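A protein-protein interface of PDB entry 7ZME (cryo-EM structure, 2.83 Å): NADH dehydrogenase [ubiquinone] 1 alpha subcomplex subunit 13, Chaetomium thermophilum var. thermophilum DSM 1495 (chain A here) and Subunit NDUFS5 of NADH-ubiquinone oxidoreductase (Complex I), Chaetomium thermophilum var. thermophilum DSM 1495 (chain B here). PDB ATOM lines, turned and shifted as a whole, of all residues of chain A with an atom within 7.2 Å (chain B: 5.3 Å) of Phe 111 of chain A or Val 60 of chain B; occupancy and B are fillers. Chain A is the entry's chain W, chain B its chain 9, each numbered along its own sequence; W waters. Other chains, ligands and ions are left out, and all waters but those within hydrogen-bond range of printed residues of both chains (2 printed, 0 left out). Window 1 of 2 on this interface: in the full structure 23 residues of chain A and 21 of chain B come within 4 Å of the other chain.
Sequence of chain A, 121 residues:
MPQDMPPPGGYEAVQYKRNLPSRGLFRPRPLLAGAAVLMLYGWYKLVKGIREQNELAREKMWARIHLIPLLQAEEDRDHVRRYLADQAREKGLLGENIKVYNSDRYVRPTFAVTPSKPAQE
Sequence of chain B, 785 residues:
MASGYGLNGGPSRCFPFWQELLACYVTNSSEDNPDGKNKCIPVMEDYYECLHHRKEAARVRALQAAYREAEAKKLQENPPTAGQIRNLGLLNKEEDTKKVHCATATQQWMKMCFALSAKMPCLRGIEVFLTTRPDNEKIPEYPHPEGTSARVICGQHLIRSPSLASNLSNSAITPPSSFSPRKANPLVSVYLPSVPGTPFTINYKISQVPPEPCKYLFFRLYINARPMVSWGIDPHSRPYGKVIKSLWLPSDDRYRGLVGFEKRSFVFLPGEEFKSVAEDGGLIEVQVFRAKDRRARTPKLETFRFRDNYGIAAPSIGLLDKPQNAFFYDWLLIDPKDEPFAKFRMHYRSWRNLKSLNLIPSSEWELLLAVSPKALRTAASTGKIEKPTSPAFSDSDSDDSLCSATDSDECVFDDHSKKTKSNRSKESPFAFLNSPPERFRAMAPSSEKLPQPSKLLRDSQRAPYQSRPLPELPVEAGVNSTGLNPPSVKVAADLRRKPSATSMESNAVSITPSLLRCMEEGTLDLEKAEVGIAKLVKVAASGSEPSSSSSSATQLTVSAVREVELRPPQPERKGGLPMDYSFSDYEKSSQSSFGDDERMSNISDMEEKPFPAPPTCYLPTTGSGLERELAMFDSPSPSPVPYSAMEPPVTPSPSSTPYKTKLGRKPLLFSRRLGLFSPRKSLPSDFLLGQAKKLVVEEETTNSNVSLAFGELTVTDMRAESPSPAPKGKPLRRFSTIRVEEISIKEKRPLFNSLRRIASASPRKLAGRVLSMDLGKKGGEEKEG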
ATOM      1  N   ASP A  86     -25.932  -4.368  -9.342  1.00  0.00           N
ATOM      2  CA  ASP A  86     -24.787  -4.970  -8.666  1.00  0.00           C
ATOM      3  C   ASP A  86     -24.903  -6.487  -8.632  1.00  0.00           C
ATOM      4  O   ASP A  86     -23.892  -7.195  -8.701  1.00  0.00           O
ATOM      5  CB  ASP A  86     -24.651  -4.404  -7.255  1.00  0.00           C
ATOM      6  CG  ASP A  86     -23.436  -4.949  -6.522  1.00  0.00           C
ATOM      7  OD1 ASP A  86     -22.305  -4.512  -6.830  1.00  0.00           O
ATOM      8  OD2 ASP A  86     -23.610  -5.814  -5.639  1.00  0.00           O
ATOM      9  N   GLU A  90     -21.923  -8.736 -10.333  1.00  0.00           N
ATOM     10  CA  GLU A  90     -21.253  -9.846  -9.620  1.00  0.00           C
ATOM     11  C   GLU A  90     -21.409 -11.132 -10.412  1.00  0.00           C
ATOM     12  O   GLU A  90     -20.426 -11.870 -10.514  1.00  0.00           O
ATOM     13  CB  GLU A  90     -21.928 -10.103  -8.280  1.00  0.00           C
ATOM     14  CG  GLU A  90     -21.112 -10.939  -7.332  1.00  0.00           C
ATOM     15  CD  GLU A  90     -21.599 -10.805  -5.906  1.00  0.00           C
ATOM     16  OE1 GLU A  90     -22.823 -10.713  -5.709  1.00  0.00           O
ATOM     17  OE2 GLU A  90     -20.753 -10.769  -5.005  1.00  0.00           O
ATOM     18  N   LEU A  94     -17.765 -12.088 -10.712  1.00  0.00           N
ATOM     19  CA  LEU A  94     -17.472 -13.192  -9.811  1.00  0.00           C
ATOM     20  C   LEU A  94     -18.134 -14.495 -10.233  1.00  0.00           C
ATOM     21  O   LEU A  94     -17.933 -15.518  -9.571  1.00  0.00           O
ATOM     22  CB  LEU A  94     -17.892 -12.838  -8.380  1.00  0.00           C
ATOM     23  CG  LEU A  94     -17.144 -11.687  -7.699  1.00  0.00           C
ATOM     24  CD1 LEU A  94     -17.709 -11.429  -6.315  1.00  0.00           C
ATOM     25  CD2 LEU A  94     -15.653 -11.952  -7.631  1.00  0.00           C
ATOM     26  N   VAL A 100     -24.415 -12.226   1.490  1.00  0.00           N
ATOM     27  CA  VAL A 100     -23.975 -11.560   2.749  1.00  0.00           C
ATOM     28  C   VAL A 100     -24.955 -11.886   3.875  1.00  0.00           C
ATOM     29  O   VAL A 100     -24.496 -12.121   4.998  1.00  0.00           O
ATOM     30  CB  VAL A 100     -23.803 -10.044   2.557  1.00  0.00           C
ATOM     31  CG1 VAL A 100     -23.416  -9.344   3.846  1.00  0.00           C
ATOM     32  CG2 VAL A 100     -22.809  -9.729   1.452  1.00  0.00           C
ATOM     33  N   ARG A 108     -29.728  -1.835   2.908  1.00  0.00           N
ATOM     34  CA  ARG A 108     -29.008  -0.733   2.227  1.00  0.00           C
ATOM     35  C   ARG A 108     -27.497  -0.950   2.341  1.00  0.00           C
ATOM     36  O   ARG A 108     -27.003  -1.122   3.466  1.00  0.00           O
ATOM     37  CB  ARG A 108     -29.449   0.610   2.815  1.00  0.00           C
ATOM     38  CG  ARG A 108     -30.787   1.095   2.282  1.00  0.00           C
ATOM     39  CD  ARG A 108     -31.551   1.926   3.288  1.00  0.00           C
ATOM     40  NE  ARG A 108     -32.868   2.309   2.803  1.00  0.00           N
ATOM     41  CZ  ARG A 108     -33.987   1.633   3.037  1.00  0.00           C
ATOM     42  NH1 ARG A 108     -35.138   2.070   2.557  1.00  0.00           N
ATOM     43  NH2 ARG A 108     -33.956   0.526   3.753  1.00  0.00           N
ATOM     44  N   PRO A 109     -26.745  -0.905   1.216  1.00  0.00           N
ATOM     45  CA  PRO A 109     -25.305  -1.192   1.228  1.00  0.00           C
ATOM     46  C   PRO A 109     -24.416  -0.273   2.075  1.00  0.00           C
ATOM     47  O   PRO A 109     -24.562   0.908   1.981  1.00  0.00           O
ATOM     48  CB  PRO A 109     -24.932  -0.932  -0.238  1.00  0.00           C
ATOM     49  CG  PRO A 109     -26.187  -1.191  -1.019  1.00  0.00           C
ATOM     50  CD  PRO A 109     -27.271  -0.646  -0.123  1.00  0.00           C
ATOM     51  N   THR A 110     -23.529  -0.841   2.890  1.00  0.00           N
ATOM     52  CA  THR A 110     -22.559  -0.041   3.690  1.00  0.00           C
ATOM     53  C   THR A 110     -21.344   0.228   2.810  1.00  0.00           C
ATOM     54  O   THR A 110     -20.672   1.241   3.015  1.00  0.00           O
ATOM     55  CB  THR A 110     -22.155  -0.831   4.940  1.00  0.00           C
ATOM     56  OG1 THR A 110     -23.348  -1.075   5.680  1.00  0.00           O
ATOM     57  CG2 THR A 110     -21.145  -0.128   5.818  1.00  0.00           C
ATOM     58  N   PHE A 111     -21.119  -0.646   1.836  1.00  0.00           N
ATOM     59  CA  PHE A 111     -19.918  -0.564   0.980  1.00  0.00           C
ATOM     60  C   PHE A 111     -20.350  -0.667  -0.475  1.00  0.00           C
ATOM     61  O   PHE A 111     -21.321  -1.382  -0.757  1.00  0.00           O
ATOM     62  CB  PHE A 111     -19.017  -1.764   1.277  1.00  0.00           C
ATOM     63  CG  PHE A 111     -18.446  -1.841   2.668  1.00  0.00           C
ATOM     64  CD1 PHE A 111     -17.415  -1.003   3.057  1.00  0.00           C
ATOM     65  CD2 PHE A 111     -18.921  -2.770   3.576  1.00  0.00           C
ATOM     66  CE1 PHE A 111     -16.880  -1.089   4.331  1.00  0.00           C
ATOM     67  CE2 PHE A 111     -18.392  -2.846   4.852  1.00  0.00           C
ATOM     68  CZ  PHE A 111     -17.371  -2.007   5.227  1.00  0.00           C
ATOM     69  N   ALA A 112     -19.633   0.004  -1.371  1.00  0.00           N
ATOM     70  CA  ALA A 112     -19.944  -0.123  -2.810  1.00  0.00           C
ATOM     71  C   ALA A 112     -18.665  -0.257  -3.624  1.00  0.00           C
ATOM     72  O   ALA A 112     -17.669   0.361  -3.238  1.00  0.00           O
ATOM     73  CB  ALA A 112     -20.746   1.055  -3.282  1.00  0.00           C
ATOM     74  N   VAL A 113     -18.693  -1.059  -4.682  1.00  0.00           N
ATOM     75  CA  VAL A 113     -17.571  -1.155  -5.604  1.00  0.00           C
ATOM     76  C   VAL A 113     -17.405   0.182  -6.313  1.00  0.00           C
ATOM     77  O   VAL A 113     -18.369   0.741  -6.848  1.00  0.00           O
ATOM     78  CB  VAL A 113     -17.798  -2.296  -6.607  1.00  0.00           C
ATOM     79  CG1 VAL A 113     -16.953  -2.093  -7.852  1.00  0.00           C
ATOM     80  CG2 VAL A 113     -17.505  -3.633  -5.972  1.00  0.00           C
ATOM     81  N   THR A 114     -16.187   0.708  -6.313  1.00  0.00           N
ATOM     82  CA  THR A 114     -15.923   1.958  -7.002  1.00  0.00           C
ATOM     83  C   THR A 114     -14.789   1.769  -7.997  1.00  0.00           C
ATOM     84  O   THR A 114     -13.928   0.903  -7.809  1.00  0.00           O
ATOM     85  CB  THR A 114     -15.558   3.088  -6.022  1.00  0.00           C
ATOM     86  OG1 THR A 114     -14.193   2.954  -5.614  1.00  0.00           O
ATOM     87  CG2 THR A 114     -16.460   3.063  -4.799  1.00  0.00           C
ATOM     88  N   HIS B  53     -20.412  -5.865   9.543  1.00  0.00           N
ATOM     89  CA  HIS B  53     -20.236  -5.791   8.064  1.00  0.00           C
ATOM     90  C   HIS B  53     -18.993  -6.532   7.547  1.00  0.00           C
ATOM     91  O   HIS B  53     -18.516  -6.142   6.480  1.00  0.00           O
ATOM     92  CB  HIS B  53     -20.210  -4.339   7.567  1.00  0.00           C
ATOM     93  CG  HIS B  53     -21.238  -3.438   8.156  1.00  0.00           C
ATOM     94  ND1 HIS B  53     -22.567  -3.503   7.803  1.00  0.00           N
ATOM     95  CD2 HIS B  53     -21.130  -2.426   9.042  1.00  0.00           C
ATOM     96  CE1 HIS B  53     -23.237  -2.583   8.459  1.00  0.00           C
ATOM     97  NE2 HIS B  53     -22.380  -1.912   9.226  1.00  0.00           N
ATOM     98  N   GLU B  56     -19.923  -8.474   4.231  1.00  0.00           N
ATOM     99  CA  GLU B  56     -20.233  -7.589   3.080  1.00  0.00           C
ATOM    100  C   GLU B  56     -18.950  -6.904   2.643  1.00  0.00           C
ATOM    101  O   GLU B  56     -18.829  -6.555   1.457  1.00  0.00           O
ATOM    102  CB  GLU B  56     -21.234  -6.504   3.462  1.00  0.00           C
ATOM    103  CG  GLU B  56     -21.662  -5.624   2.306  1.00  0.00           C
ATOM    104  CD  GLU B  56     -22.210  -4.262   2.699  1.00  0.00           C
ATOM    105  OE1 GLU B  56     -22.553  -4.079   3.884  1.00  0.00           O
ATOM    106  OE2 GLU B  56     -22.288  -3.386   1.820  1.00  0.00           O
ATOM    107  N   ALA B  57     -18.017  -6.745   3.579  1.00  0.00           N
ATOM    108  CA  ALA B  57     -16.762  -6.062   3.222  1.00  0.00           C
ATOM    109  C   ALA B  57     -15.930  -7.061   2.435  1.00  0.00           C
ATOM    110  O   ALA B  57     -15.171  -6.646   1.548  1.00  0.00           O
ATOM    111  CB  ALA B  57     -16.050  -5.655   4.483  1.00  0.00           C
ATOM    112  N   ALA B  58     -16.105  -8.338   2.755  1.00  0.00           N
ATOM    113  CA  ALA B  58     -15.398  -9.370   2.008  1.00  0.00           C
ATOM    114  C   ALA B  58     -15.988  -9.546   0.616  1.00  0.00           C
ATOM    115  O   ALA B  58     -15.258  -9.817  -0.342  1.00  0.00           O
ATOM    116  CB  ALA B  58     -15.426 -10.685   2.778  1.00  0.00           C
ATOM    117  N   ARG B  59     -17.306  -9.400   0.484  1.00  0.00           N
ATOM    118  CA  ARG B  59     -17.928  -9.518  -0.830  1.00  0.00           C
ATOM    119  C   ARG B  59     -17.511  -8.374  -1.742  1.00  0.00           C
ATOM    120  O   ARG B  59     -17.098  -8.597  -2.885  1.00  0.00           O
ATOM    121  CB  ARG B  59     -19.445  -9.557  -0.699  1.00  0.00           C
ATOM    122  CG  ARG B  59     -20.135  -9.903  -2.000  1.00  0.00           C
ATOM    123  CD  ARG B  59     -21.556  -9.387  -2.026  1.00  0.00           C
ATOM    124  NE  ARG B  59     -21.594  -7.941  -2.204  1.00  0.00           N
ATOM    125  CZ  ARG B  59     -22.014  -7.335  -3.306  1.00  0.00           C
ATOM    126  NH1 ARG B  59     -22.446  -8.049  -4.333  1.00  0.00           N
ATOM    127  NH2 ARG B  59     -22.013  -6.013  -3.378  1.00  0.00           N
ATOM    128  N   VAL B  60     -17.621  -7.138  -1.255  1.00  0.00           N
ATOM    129  CA  VAL B  60     -17.257  -5.983  -2.068  1.00  0.00           C
ATOM    130  C   VAL B  60     -15.775  -6.020  -2.406  1.00  0.00           C
ATOM    131  O   VAL B  60     -15.371  -5.690  -3.524  1.00  0.00           O
ATOM    132  CB  VAL B  60     -17.654  -4.679  -1.349  1.00  0.00           C
ATOM    133  CG1 VAL B  60     -16.971  -3.483  -1.980  1.00  0.00           C
ATOM    134  CG2 VAL B  60     -19.161  -4.501  -1.380  1.00  0.00           C
ATOM    135  N   ARG B  61     -14.943  -6.451  -1.454  1.00  0.00           N
ATOM    136  CA  ARG B  61     -13.505  -6.527  -1.695  1.00  0.00           C
ATOM    137  C   ARG B  61     -13.187  -7.449  -2.865  1.00  0.00           C
ATOM    138  O   ARG B  61     -12.435  -7.080  -3.773  1.00  0.00           O
ATOM    139  CB  ARG B  61     -12.787  -6.998  -0.431  1.00  0.00           C
ATOM    140  CG  ARG B  61     -11.435  -6.351  -0.213  1.00  0.00           C
ATOM    141  CD  ARG B  61     -10.782  -6.842   1.068  1.00  0.00           C
ATOM    142  NE  ARG B  61     -11.648  -6.681   2.232  1.00  0.00           N
ATOM    143  CZ  ARG B  61     -11.697  -5.583   2.979  1.00  0.00           C
ATOM    144  NH1 ARG B  61     -10.932  -4.542   2.685  1.00  0.00           N
ATOM    145  NH2 ARG B  61     -12.513  -5.525   4.019  1.00  0.00           N
ATOM    146  N   ALA B  62     -13.748  -8.659  -2.857  1.00  0.00           N
ATOM    147  CA  ALA B  62     -13.548  -9.576  -3.975  1.00  0.00           C
ATOM    148  C   ALA B  62     -14.149  -9.025  -5.260  1.00  0.00           C
ATOM    149  O   ALA B  62     -13.535  -9.114  -6.328  1.00  0.00           O
ATOM    150  CB  ALA B  62     -14.151 -10.940  -3.648  1.00  0.00           C
ATOM    151  N   LEU B  63     -15.348  -8.452  -5.177  1.00  0.00           N
ATOM    152  CA  LEU B  63     -15.999  -7.906  -6.360  1.00  0.00           C
ATOM    153  C   LEU B  63     -15.280  -6.671  -6.888  1.00  0.00           C
ATOM    154  O   LEU B  63     -15.269  -6.437  -8.099  1.00  0.00           O
ATOM    155  CB  LEU B  63     -17.458  -7.582  -6.038  1.00  0.00           C
ATOM    156  CG  LEU B  63     -18.422  -7.311  -7.194  1.00  0.00           C
ATOM    157  CD1 LEU B  63     -18.259  -8.338  -8.295  1.00  0.00           C
ATOM    158  CD2 LEU B  63     -19.854  -7.285  -6.688  1.00  0.00           C
ATOM    159  N   GLN B  64     -14.677  -5.872  -6.007  1.00  0.00           N
ATOM    160  CA  GLN B  64     -14.036  -4.639  -6.452  1.00  0.00           C
ATOM    161  C   GLN B  64     -12.696  -4.900  -7.125  1.00  0.00           C
ATOM    162  O   GLN B  64     -12.346  -4.207  -8.085  1.00  0.00           O
ATOM    163  CB  GLN B  64     -13.860  -3.684  -5.273  1.00  0.00           C
ATOM    164  CG  GLN B  64     -13.290  -2.333  -5.637  1.00  0.00           C
ATOM    165  CD  GLN B  64     -13.197  -1.424  -4.443  1.00  0.00           C
ATOM    166  OE1 GLN B  64     -13.524  -1.820  -3.328  1.00  0.00           O
ATOM    167  NE2 GLN B  64     -12.784  -0.189  -4.668  1.00  0.00           N
ATOM    168  N   ALA B  65     -11.929  -5.874  -6.636  1.00  0.00           N
ATOM    169  CA  ALA B  65     -10.694  -6.238  -7.319  1.00  0.00           C
ATOM    170  C   ALA B  65     -10.992  -6.919  -8.646  1.00  0.00           C
ATOM    171  O   ALA B  65     -10.292  -6.693  -9.639  1.00  0.00           O
ATOM    172  CB  ALA B  65      -9.843  -7.138  -6.427  1.00  0.00           C
HETATM  173  O   HOH W   1     -25.422  -2.692   5.143  1.00  0.00           O
HETATM  174  O   HOH W   2     -15.073   0.421  -2.502  1.00  0.00           O
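Of the 11 printed residues of chain B, 8 touch a printed residue of chain A. Printed residues of chain B that touch a printed residue of chain A: His 53, Glu 56, Ala 57, Arg 59, Val 60, Ala 62, Leu 63 and Gln 64. Of the 11 printed residues of chain A, 10 touch a printed residue of chain B. Hydrophobic or aromatic side chains of chain A that line the printed part of chain B: Leu 94, Val 100, Phe 111 and Val 113. Among the printed residues, 20 pairs touch across the chains. Among the printed residues, Asp or Glu carboxylates within 4 Å of a Lys or Arg side-chain nitrogen of the other chain: Asp 86 of chain A with Arg 59 of chain B and Glu 90 of chain A with Arg 59 of chain B.
The guanidinium group (NH1) of Arg 59 of chain B is in salt-bridge range of the side-chain carboxylate (OE1) of Glu 90 of chain A. OE2 of Glu 56 of chain B lies within hydrogen-bond range of N of Phe 111 of chain A (3.0 Å). The backbone NH (N) of Thr 110 of chain A sits at hydrogen-bond distance from the side-chain carboxylate (OE2) of Glu 56 of chain B (3.0 Å). The side-chain carboxylate (OD2) of Asp 86 of chain A lies within salt-bridge range of the guanidinium group (NH2) of Arg 59 of chain B, 2.8 Å away. OG1 of Thr 110 of chain A lies close to ND1 of His 53 of chain B, 3.3 Å away.
Phe 111 of chain A touches just these residues of chain B: His 53 (3.6 Å), Glu 56 (3.0 Å), Ala 57 (3.7 Å) and Val 60 (3.8 Å). Printed residues of chain A within 4 Å of Val 60 of chain B: Phe 111 (3.8 Å), Ala 112 (3.997 Å) and Val 113 (3.8 Å). Printed residues of chain B within 4 Å of Glu 90 of chain A: Arg 59 and Leu 63. Of the printed residues of chain A, His 53 of chain B touches Thr 110 and Phe 111. Of the printed residues of chain A, Ala 62 of chain B touches Leu 94. Of the printed residues of chain B, Val 100 of chain A touches Glu 56 (3.6 Å) and Arg 59 (3.7 Å). The nearest printed residue of chain B that does not touch Phe 111 of chain A is Arg 59 of chain B (5.4 Å). The nearest printed residue of chain A that does not touch Val 60 of chain B is Thr 114 of chain A (6.1 Å).
Asp 86 of chain A touches Leu 63 of chain B. Ala 62 of chain B touches Leu 94 of chain A. Leu 94 of chain A touches Leu 63 of chain B (CG to CD1, 3.6 Å). Glu 56 of chain B touches Val 100 of chain A. Pro 109 of chain A touches Glu 56 of chain B (CA to OE2, 3.8 Å). Phe 111 of chain A touches Ala 57 of chain B. CB of Phe 111 of chain A touches CG2 of Val 60 of chain B, 3.8 Å away. Val 113 of chain A touches Val 60 of chain B (CG2 to O, 3.8 Å). Val 113 of chain A touches Gln 64 of chain B (CG2 to N, 3.6 Å). Gln 64 of chain B touches Thr 114 of chain A (NE2 to O, 3.5 Å).
Water W1 lies within hydrogen-bond range of OG1 of Thr 110 of chain A (2.7 Å), O of Arg 108 of chain A (2.8 Å) and OE1 of Glu 56 of chain B (3.4 Å). Water W2 bridges the backbone carbonyl oxygen (O) of Ala 112 of chain A (2.7 Å) and the side-chain amide oxygen (OE1) of Gln 64 of chain B (2.8 Å).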
